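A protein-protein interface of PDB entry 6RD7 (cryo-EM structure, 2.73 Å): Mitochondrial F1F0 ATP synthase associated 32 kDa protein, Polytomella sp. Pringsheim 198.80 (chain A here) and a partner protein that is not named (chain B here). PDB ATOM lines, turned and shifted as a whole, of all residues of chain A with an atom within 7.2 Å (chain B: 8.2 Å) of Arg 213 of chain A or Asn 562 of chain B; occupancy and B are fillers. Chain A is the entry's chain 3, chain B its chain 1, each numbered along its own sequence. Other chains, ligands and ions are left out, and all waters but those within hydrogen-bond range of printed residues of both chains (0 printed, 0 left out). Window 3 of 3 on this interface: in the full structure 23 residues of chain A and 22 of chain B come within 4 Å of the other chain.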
ATOM      1  N   GLU A 175      26.085  -6.779   2.475  1.00  0.00           N
ATOM      2  CA  GLU A 175      25.136  -7.390   3.399  1.00  0.00           C
ATOM      3  C   GLU A 175      24.778  -8.810   2.980  1.00  0.00           C
ATOM      4  O   GLU A 175      24.555  -9.670   3.836  1.00  0.00           O
ATOM      5  CB  GLU A 175      23.860  -6.542   3.477  1.00  0.00           C
ATOM      6  CG  GLU A 175      23.933  -5.164   4.178  1.00  0.00           C
ATOM      7  CD  GLU A 175      24.884  -4.152   3.534  1.00  0.00           C
ATOM      8  OE1 GLU A 175      24.857  -4.003   2.292  1.00  0.00           O
ATOM      9  OE2 GLU A 175      25.646  -3.495   4.277  1.00  0.00           O
ATOM     10  N   LEU A 178      28.461 -11.150   2.802  1.00  0.00           N
ATOM     11  CA  LEU A 178      28.922 -11.681   4.077  1.00  0.00           C
ATOM     12  C   LEU A 178      28.188 -12.962   4.444  1.00  0.00           C
ATOM     13  O   LEU A 178      28.815 -13.927   4.896  1.00  0.00           O
ATOM     14  CB  LEU A 178      28.755 -10.628   5.164  1.00  0.00           C
ATOM     15  CG  LEU A 178      29.805  -9.528   5.071  1.00  0.00           C
ATOM     16  CD1 LEU A 178      29.341  -8.298   5.793  1.00  0.00           C
ATOM     17  CD2 LEU A 178      31.087 -10.027   5.658  1.00  0.00           C
ATOM     18  N   LEU A 209      31.356   2.337   3.537  1.00  0.00           N
ATOM     19  CA  LEU A 209      30.848   2.246   4.897  1.00  0.00           C
ATOM     20  C   LEU A 209      29.926   1.058   5.103  1.00  0.00           C
ATOM     21  O   LEU A 209      29.277   0.976   6.147  1.00  0.00           O
ATOM     22  CB  LEU A 209      30.107   3.522   5.270  1.00  0.00           C
ATOM     23  CG  LEU A 209      30.918   4.805   5.291  1.00  0.00           C
ATOM     24  CD1 LEU A 209      29.978   5.939   5.543  1.00  0.00           C
ATOM     25  CD2 LEU A 209      31.982   4.742   6.356  1.00  0.00           C
ATOM     26  N   ALA A 210      29.827   0.158   4.136  1.00  0.00           N
ATOM     27  CA  ALA A 210      29.041  -1.058   4.331  1.00  0.00           C
ATOM     28  C   ALA A 210      29.618  -2.034   5.360  1.00  0.00           C
ATOM     29  O   ALA A 210      28.818  -2.735   6.002  1.00  0.00           O
ATOM     30  CB  ALA A 210      28.812  -1.741   2.980  1.00  0.00           C
ATOM     31  N   PRO A 211      30.942  -2.168   5.565  1.00  0.00           N
ATOM     32  CA  PRO A 211      31.396  -2.953   6.727  1.00  0.00           C
ATOM     33  C   PRO A 211      31.067  -2.342   8.078  1.00  0.00           C
ATOM     34  O   PRO A 211      31.076  -3.067   9.077  1.00  0.00           O
ATOM     35  CB  PRO A 211      32.909  -3.037   6.517  1.00  0.00           C
ATOM     36  CG  PRO A 211      33.050  -3.032   5.097  1.00  0.00           C
ATOM     37  CD  PRO A 211      32.065  -2.042   4.609  1.00  0.00           C
ATOM     38  N   VAL A 212      30.800  -1.036   8.148  1.00  0.00           N
ATOM     39  CA  VAL A 212      30.400  -0.414   9.401  1.00  0.00           C
ATOM     40  C   VAL A 212      29.027  -0.904   9.853  1.00  0.00           C
ATOM     41  O   VAL A 212      28.789  -1.071  11.055  1.00  0.00           O
ATOM     42  CB  VAL A 212      30.453   1.116   9.226  1.00  0.00           C
ATOM     43  CG1 VAL A 212      30.052   1.835  10.479  1.00  0.00           C
ATOM     44  CG2 VAL A 212      31.842   1.541   8.806  1.00  0.00           C
ATOM     45  N   ARG A 213      28.135  -1.201   8.912  1.00  0.00           N
ATOM     46  CA  ARG A 213      26.785  -1.658   9.207  1.00  0.00           C
ATOM     47  C   ARG A 213      26.688  -3.177   9.289  1.00  0.00           C
ATOM     48  O   ARG A 213      25.589  -3.731   9.293  1.00  0.00           O
ATOM     49  CB  ARG A 213      25.815  -1.138   8.150  1.00  0.00           C
ATOM     50  CG  ARG A 213      25.432   0.304   8.320  1.00  0.00           C
ATOM     51  CD  ARG A 213      24.135   0.424   9.084  1.00  0.00           C
ATOM     52  NE  ARG A 213      23.522   1.728   8.888  1.00  0.00           N
ATOM     53  CZ  ARG A 213      23.823   2.801   9.605  1.00  0.00           C
ATOM     54  NH1 ARG A 213      23.223   3.957   9.363  1.00  0.00           N
ATOM     55  NH2 ARG A 213      24.724   2.713  10.570  1.00  0.00           N
ATOM     56  N   ALA A 214      27.822  -3.865   9.366  1.00  0.00           N
ATOM     57  CA  ALA A 214      27.859  -5.305   9.149  1.00  0.00           C
ATOM     58  C   ALA A 214      27.744  -6.127  10.422  1.00  0.00           C
ATOM     59  O   ALA A 214      27.039  -7.138  10.434  1.00  0.00           O
ATOM     60  CB  ALA A 214      29.150  -5.692   8.429  1.00  0.00           C
ATOM     61  N   GLY A 215      28.410  -5.730  11.487  1.00  0.00           N
ATOM     62  CA  GLY A 215      28.528  -6.644  12.608  1.00  0.00           C
ATOM     63  C   GLY A 215      29.886  -7.311  12.513  1.00  0.00           C
ATOM     64  O   GLY A 215      30.282  -7.807  11.453  1.00  0.00           O
ATOM     65  N   ALA A 216      30.609  -7.324  13.633  1.00  0.00           N
ATOM     66  CA  ALA A 216      32.023  -7.677  13.590  1.00  0.00           C
ATOM     67  C   ALA A 216      32.228  -9.177  13.418  1.00  0.00           C
ATOM     68  O   ALA A 216      33.300  -9.612  12.979  1.00  0.00           O
ATOM     69  CB  ALA A 216      32.724  -7.178  14.850  1.00  0.00           C
ATOM     70  N   GLU A 218      30.570 -11.183  11.286  1.00  0.00           N
ATOM     71  CA  GLU A 218      30.548 -11.497   9.863  1.00  0.00           C
ATOM     72  C   GLU A 218      31.834 -11.052   9.181  1.00  0.00           C
ATOM     73  O   GLU A 218      32.356 -11.750   8.301  1.00  0.00           O
ATOM     74  CB  GLU A 218      29.339 -10.837   9.211  1.00  0.00           C
ATOM     75  CG  GLU A 218      28.023 -11.436   9.643  1.00  0.00           C
ATOM     76  CD  GLU A 218      26.845 -10.856   8.894  1.00  0.00           C
ATOM     77  OE1 GLU A 218      26.710  -9.616   8.864  1.00  0.00           O
ATOM     78  OE2 GLU A 218      26.049 -11.640   8.338  1.00  0.00           O
ATOM     79  N   LEU A 219      32.370  -9.901   9.590  1.00  0.00           N
ATOM     80  CA  LEU A 219      33.645  -9.445   9.055  1.00  0.00           C
ATOM     81  C   LEU A 219      34.781 -10.352   9.503  1.00  0.00           C
ATOM     82  O   LEU A 219      35.710 -10.615   8.732  1.00  0.00           O
ATOM     83  CB  LEU A 219      33.907  -8.005   9.483  1.00  0.00           C
ATOM     84  CG  LEU A 219      32.811  -6.989   9.180  1.00  0.00           C
ATOM     85  CD1 LEU A 219      33.023  -5.758  10.020  1.00  0.00           C
ATOM     86  CD2 LEU A 219      32.803  -6.637   7.709  1.00  0.00           C
ATOM     87  N   GLY A 243      35.408  -1.885   9.282  1.00  0.00           N
ATOM     88  CA  GLY A 243      34.184  -2.223   9.986  1.00  0.00           C
ATOM     89  C   GLY A 243      34.399  -2.573  11.446  1.00  0.00           C
ATOM     90  O   GLY A 243      33.449  -2.611  12.229  1.00  0.00           O
ATOM     91  N   SER A 248      30.977  -1.712  16.880  1.00  0.00           N
ATOM     92  CA  SER A 248      30.599  -3.003  16.315  1.00  0.00           C
ATOM     93  C   SER A 248      30.977  -4.149  17.242  1.00  0.00           C
ATOM     94  O   SER A 248      30.250  -5.144  17.341  1.00  0.00           O
ATOM     95  CB  SER A 248      31.250  -3.179  14.947  1.00  0.00           C
ATOM     96  OG  SER A 248      32.658  -3.180  15.056  1.00  0.00           O
ATOM     97  N   LYS A 251      28.530  -4.138  20.187  1.00  0.00           N
ATOM     98  CA  LYS A 251      27.232  -4.751  19.916  1.00  0.00           C
ATOM     99  C   LYS A 251      27.260  -6.255  20.159  1.00  0.00           C
ATOM    100  O   LYS A 251      26.210  -6.880  20.345  1.00  0.00           O
ATOM    101  CB  LYS A 251      26.798  -4.453  18.483  1.00  0.00           C
ATOM    102  CG  LYS A 251      26.410  -3.013  18.241  1.00  0.00           C
ATOM    103  CD  LYS A 251      25.537  -2.883  17.013  1.00  0.00           C
ATOM    104  CE  LYS A 251      25.298  -1.426  16.667  1.00  0.00           C
ATOM    105  NZ  LYS A 251      26.470  -0.831  15.977  1.00  0.00           N
ATOM    106  N   LYS B 554      24.106   2.870  -7.099  1.00  0.00           N
ATOM    107  CA  LYS B 554      23.960   1.843  -6.071  1.00  0.00           C
ATOM    108  C   LYS B 554      24.531   2.297  -4.730  1.00  0.00           C
ATOM    109  O   LYS B 554      23.928   2.057  -3.679  1.00  0.00           O
ATOM    110  CB  LYS B 554      24.640   0.560  -6.541  1.00  0.00           C
ATOM    111  CG  LYS B 554      24.588  -0.590  -5.574  1.00  0.00           C
ATOM    112  CD  LYS B 554      25.739  -1.534  -5.819  1.00  0.00           C
ATOM    113  CE  LYS B 554      25.534  -2.852  -5.116  1.00  0.00           C
ATOM    114  NZ  LYS B 554      26.638  -3.787  -5.421  1.00  0.00           N
ATOM    115  N   LYS B 555      25.669   2.990  -4.749  1.00  0.00           N
ATOM    116  CA  LYS B 555      26.266   3.468  -3.504  1.00  0.00           C
ATOM    117  C   LYS B 555      25.471   4.623  -2.899  1.00  0.00           C
ATOM    118  O   LYS B 555      25.302   4.692  -1.673  1.00  0.00           O
ATOM    119  CB  LYS B 555      27.708   3.884  -3.750  1.00  0.00           C
ATOM    120  CG  LYS B 555      28.624   2.732  -4.051  1.00  0.00           C
ATOM    121  CD  LYS B 555      29.889   3.216  -4.698  1.00  0.00           C
ATOM    122  CE  LYS B 555      30.670   2.069  -5.259  1.00  0.00           C
ATOM    123  NZ  LYS B 555      32.112   2.379  -5.317  1.00  0.00           N
ATOM    124  N   ILE B 556      24.969   5.533  -3.737  1.00  0.00           N
ATOM    125  CA  ILE B 556      24.132   6.626  -3.246  1.00  0.00           C
ATOM    126  C   ILE B 556      22.814   6.083  -2.701  1.00  0.00           C
ATOM    127  O   ILE B 556      22.295   6.560  -1.683  1.00  0.00           O
ATOM    128  CB  ILE B 556      23.920   7.665  -4.365  1.00  0.00           C
ATOM    129  CG1 ILE B 556      25.235   8.357  -4.699  1.00  0.00           C
ATOM    130  CG2 ILE B 556      22.929   8.727  -3.967  1.00  0.00           C
ATOM    131  CD1 ILE B 556      25.213   9.055  -6.019  1.00  0.00           C
ATOM    132  N   ASP B 557      22.284   5.038  -3.336  1.00  0.00           N
ATOM    133  CA  ASP B 557      21.072   4.400  -2.843  1.00  0.00           C
ATOM    134  C   ASP B 557      21.329   3.658  -1.541  1.00  0.00           C
ATOM    135  O   ASP B 557      20.432   3.556  -0.699  1.00  0.00           O
ATOM    136  CB  ASP B 557      20.518   3.451  -3.900  1.00  0.00           C
ATOM    137  CG  ASP B 557      19.790   4.174  -5.009  1.00  0.00           C
ATOM    138  OD1 ASP B 557      19.649   5.410  -4.925  1.00  0.00           O
ATOM    139  OD2 ASP B 557      19.363   3.508  -5.972  1.00  0.00           O
ATOM    140  N   TRP B 558      22.539   3.122  -1.361  1.00  0.00           N
ATOM    141  CA  TRP B 558      22.897   2.544  -0.069  1.00  0.00           C
ATOM    142  C   TRP B 558      22.932   3.609   1.011  1.00  0.00           C
ATOM    143  O   TRP B 558      22.527   3.357   2.149  1.00  0.00           O
ATOM    144  CB  TRP B 558      24.253   1.839  -0.138  1.00  0.00           C
ATOM    145  CG  TRP B 558      24.610   1.129   1.148  1.00  0.00           C
ATOM    146  CD1 TRP B 558      24.342  -0.164   1.458  1.00  0.00           C
ATOM    147  CD2 TRP B 558      25.280   1.682   2.295  1.00  0.00           C
ATOM    148  NE1 TRP B 558      24.801  -0.457   2.715  1.00  0.00           N
ATOM    149  CE2 TRP B 558      25.379   0.661   3.250  1.00  0.00           C
ATOM    150  CE3 TRP B 558      25.799   2.943   2.604  1.00  0.00           C
ATOM    151  CZ2 TRP B 558      25.974   0.856   4.485  1.00  0.00           C
ATOM    152  CZ3 TRP B 558      26.387   3.133   3.828  1.00  0.00           C
ATOM    153  CH2 TRP B 558      26.474   2.097   4.754  1.00  0.00           C
ATOM    154  N   GLU B 559      23.464   4.787   0.681  1.00  0.00           N
ATOM    155  CA  GLU B 559      23.506   5.884   1.644  1.00  0.00           C
ATOM    156  C   GLU B 559      22.109   6.341   2.033  1.00  0.00           C
ATOM    157  O   GLU B 559      21.844   6.611   3.209  1.00  0.00           O
ATOM    158  CB  GLU B 559      24.291   7.056   1.071  1.00  0.00           C
ATOM    159  CG  GLU B 559      25.714   7.119   1.521  1.00  0.00           C
ATOM    160  CD  GLU B 559      26.456   8.277   0.905  1.00  0.00           C
ATOM    161  OE1 GLU B 559      26.591   9.320   1.572  1.00  0.00           O
ATOM    162  OE2 GLU B 559      26.897   8.153  -0.253  1.00  0.00           O
ATOM    163  N   THR B 560      21.206   6.440   1.059  1.00  0.00           N
ATOM    164  CA  THR B 560      19.834   6.843   1.353  1.00  0.00           C
ATOM    165  C   THR B 560      19.098   5.762   2.135  1.00  0.00           C
ATOM    166  O   THR B 560      18.313   6.066   3.039  1.00  0.00           O
ATOM    167  CB  THR B 560      19.105   7.174   0.051  1.00  0.00           C
ATOM    168  OG1 THR B 560      19.845   8.164  -0.668  1.00  0.00           O
ATOM    169  CG2 THR B 560      17.714   7.710   0.315  1.00  0.00           C
ATOM    170  N   THR B 561      19.371   4.492   1.827  1.00  0.00           N
ATOM    171  CA  THR B 561      18.691   3.387   2.495  1.00  0.00           C
ATOM    172  C   THR B 561      19.119   3.261   3.950  1.00  0.00           C
ATOM    173  O   THR B 561      18.305   2.932   4.819  1.00  0.00           O
ATOM    174  CB  THR B 561      18.969   2.084   1.748  1.00  0.00           C
ATOM    175  OG1 THR B 561      18.844   2.305   0.342  1.00  0.00           O
ATOM    176  CG2 THR B 561      17.993   1.015   2.149  1.00  0.00           C
ATOM    177  N   ASN B 562      20.388   3.531   4.239  1.00  0.00           N
ATOM    178  CA  ASN B 562      20.936   3.339   5.572  1.00  0.00           C
ATOM    179  C   ASN B 562      20.922   4.608   6.404  1.00  0.00           C
ATOM    180  O   ASN B 562      21.747   4.737   7.315  1.00  0.00           O
ATOM    181  CB  ASN B 562      22.355   2.785   5.475  1.00  0.00           C
ATOM    182  CG  ASN B 562      22.373   1.335   5.078  1.00  0.00           C
ATOM    183  OD1 ASN B 562      22.251   1.003   3.906  1.00  0.00           O
ATOM    184  ND2 ASN B 562      22.508   0.458   6.058  1.00  0.00           N
ATOM    185  N   ALA B 563      20.013   5.540   6.091  1.00  0.00           N
ATOM    186  CA  ALA B 563      19.769   6.774   6.849  1.00  0.00           C
ATOM    187  C   ALA B 563      21.016   7.646   6.943  1.00  0.00           C
ATOM    188  O   ALA B 563      21.238   8.351   7.927  1.00  0.00           O
ATOM    189  CB  ALA B 563      19.202   6.474   8.238  1.00  0.00           C
ATOM    190  N   LEU B 564      21.838   7.597   5.903  1.00  0.00           N
ATOM    191  CA  LEU B 564      23.039   8.412   5.802  1.00  0.00           C
ATOM    192  C   LEU B 564      22.947   9.359   4.619  1.00  0.00           C
ATOM    193  O   LEU B 564      23.943   9.615   3.945  1.00  0.00           O
ATOM    194  CB  LEU B 564      24.283   7.537   5.680  1.00  0.00           C
ATOM    195  CG  LEU B 564      24.672   6.721   6.904  1.00  0.00           C
ATOM    196  CD1 LEU B 564      25.583   5.592   6.490  1.00  0.00           C
ATOM    197  CD2 LEU B 564      25.344   7.605   7.928  1.00  0.00           C
ATOM    198  N   GLU B 565      21.749   9.876   4.346  1.00  0.00           N
ATOM    199  CA  GLU B 565      21.576  10.774   3.215  1.00  0.00           C
ATOM    200  C   GLU B 565      22.230  12.127   3.454  1.00  0.00           C
ATOM    201  O   GLU B 565      22.593  12.807   2.492  1.00  0.00           O
ATOM    202  CB  GLU B 565      20.091  10.938   2.895  1.00  0.00           C
ATOM    203  CG  GLU B 565      19.289  11.648   3.959  1.00  0.00           C
ATOM    204  CD  GLU B 565      18.617  10.687   4.910  1.00  0.00           C
ATOM    205  OE1 GLU B 565      18.861   9.472   4.797  1.00  0.00           O
ATOM    206  OE2 GLU B 565      17.848  11.148   5.774  1.00  0.00           O
ATOM    207  N   ASP B 566      22.440  12.508   4.708  1.00  0.00           N
ATOM    208  CA  ASP B 566      23.117  13.748   5.044  1.00  0.00           C
ATOM    209  C   ASP B 566      24.564  13.516   5.443  1.00  0.00           C
ATOM    210  O   ASP B 566      25.094  14.257   6.275  1.00  0.00           O
ATOM    211  CB  ASP B 566      22.370  14.460   6.168  1.00  0.00           C
ATOM    212  CG  ASP B 566      22.198  13.583   7.397  1.00  0.00           C
ATOM    213  OD1 ASP B 566      21.942  12.373   7.241  1.00  0.00           O
ATOM    214  OD2 ASP B 566      22.320  14.101   8.525  1.00  0.00           O
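Of the 15 printed residues of chain A, 4 touch a printed residue of chain B.
Hydrophobic or aromatic side chains of chain A within 4 Å of the printed part of chain B: Leu 209.
Along chain B the printed residues that touch a printed residue of chain A span positions 558 to 564.
Among the printed residues, 6 pairs touch across the chains.
Among the printed residues, no Asp or Glu carboxylate lies within 4 Å of a Lys or Arg side-chain nitrogen of the other chain.
Among the printed residues, pairs that only touch across the chains: Leu 209 of chain A with Trp 558 of chain B (3.3 Å), Glu 175 of chain A with Trp 558 of chain B (3.5 Å), Ala 210 of chain A with Trp 558 of chain B (3.6 Å), Arg 213 of chain A with Trp 558 of chain B (3.9 Å) and Arg 213 of chain A with Leu 564 of chain B (3.97 Å).
The backbone carbonyl oxygen (O) of Trp 558 of chain B sits close to the side-chain amide oxygen (OD1) of Asn 562 of chain B, at 3.0 Å.
The backbone carbonyl oxygen (O) of Glu 559 of chain B lies within hydrogen-bond range of the backbone NH (N) of Leu 564 of chain B (2.9 Å).
O of Asn 562 of chain B is in hydrogen-bond range of NH1 of Arg 213 of chain A.
Of the printed residues of chain B, Leu 209 of chain A touches Trp 558.
Printed residues of chain B within 4 Å of Ala 210 of chain A: Trp 558.
Of chain B, only Trp 558 (3.9 Å), Asn 562 (2.6 Å) and Leu 564 (3.97 Å) come within 4 Å of Arg 213 of chain A.
Leu 219 of chain A touches none of the printed residues of chain B.
Gly 243 of chain A touches none of the printed residues of chain B.
Printed residues of chain A within 4 Å of Trp 558 of chain B: Glu 175, Leu 209, Ala 210 and Arg 213.
Asn 562 of chain B touches just one residue of chain A: Arg 213 (2.6 Å).
Printed residues of chain A within 4 Å of Leu 564 of chain B: Arg 213 (3.97 Å).
The nearest residue of chain A that does not touch Asn 562 of chain B is Glu 175 of chain A (5.4 Å).
The nearest printed residue of chain B that does not touch Leu 209 of chain A is Leu 564 of chain B (4.5 Å).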
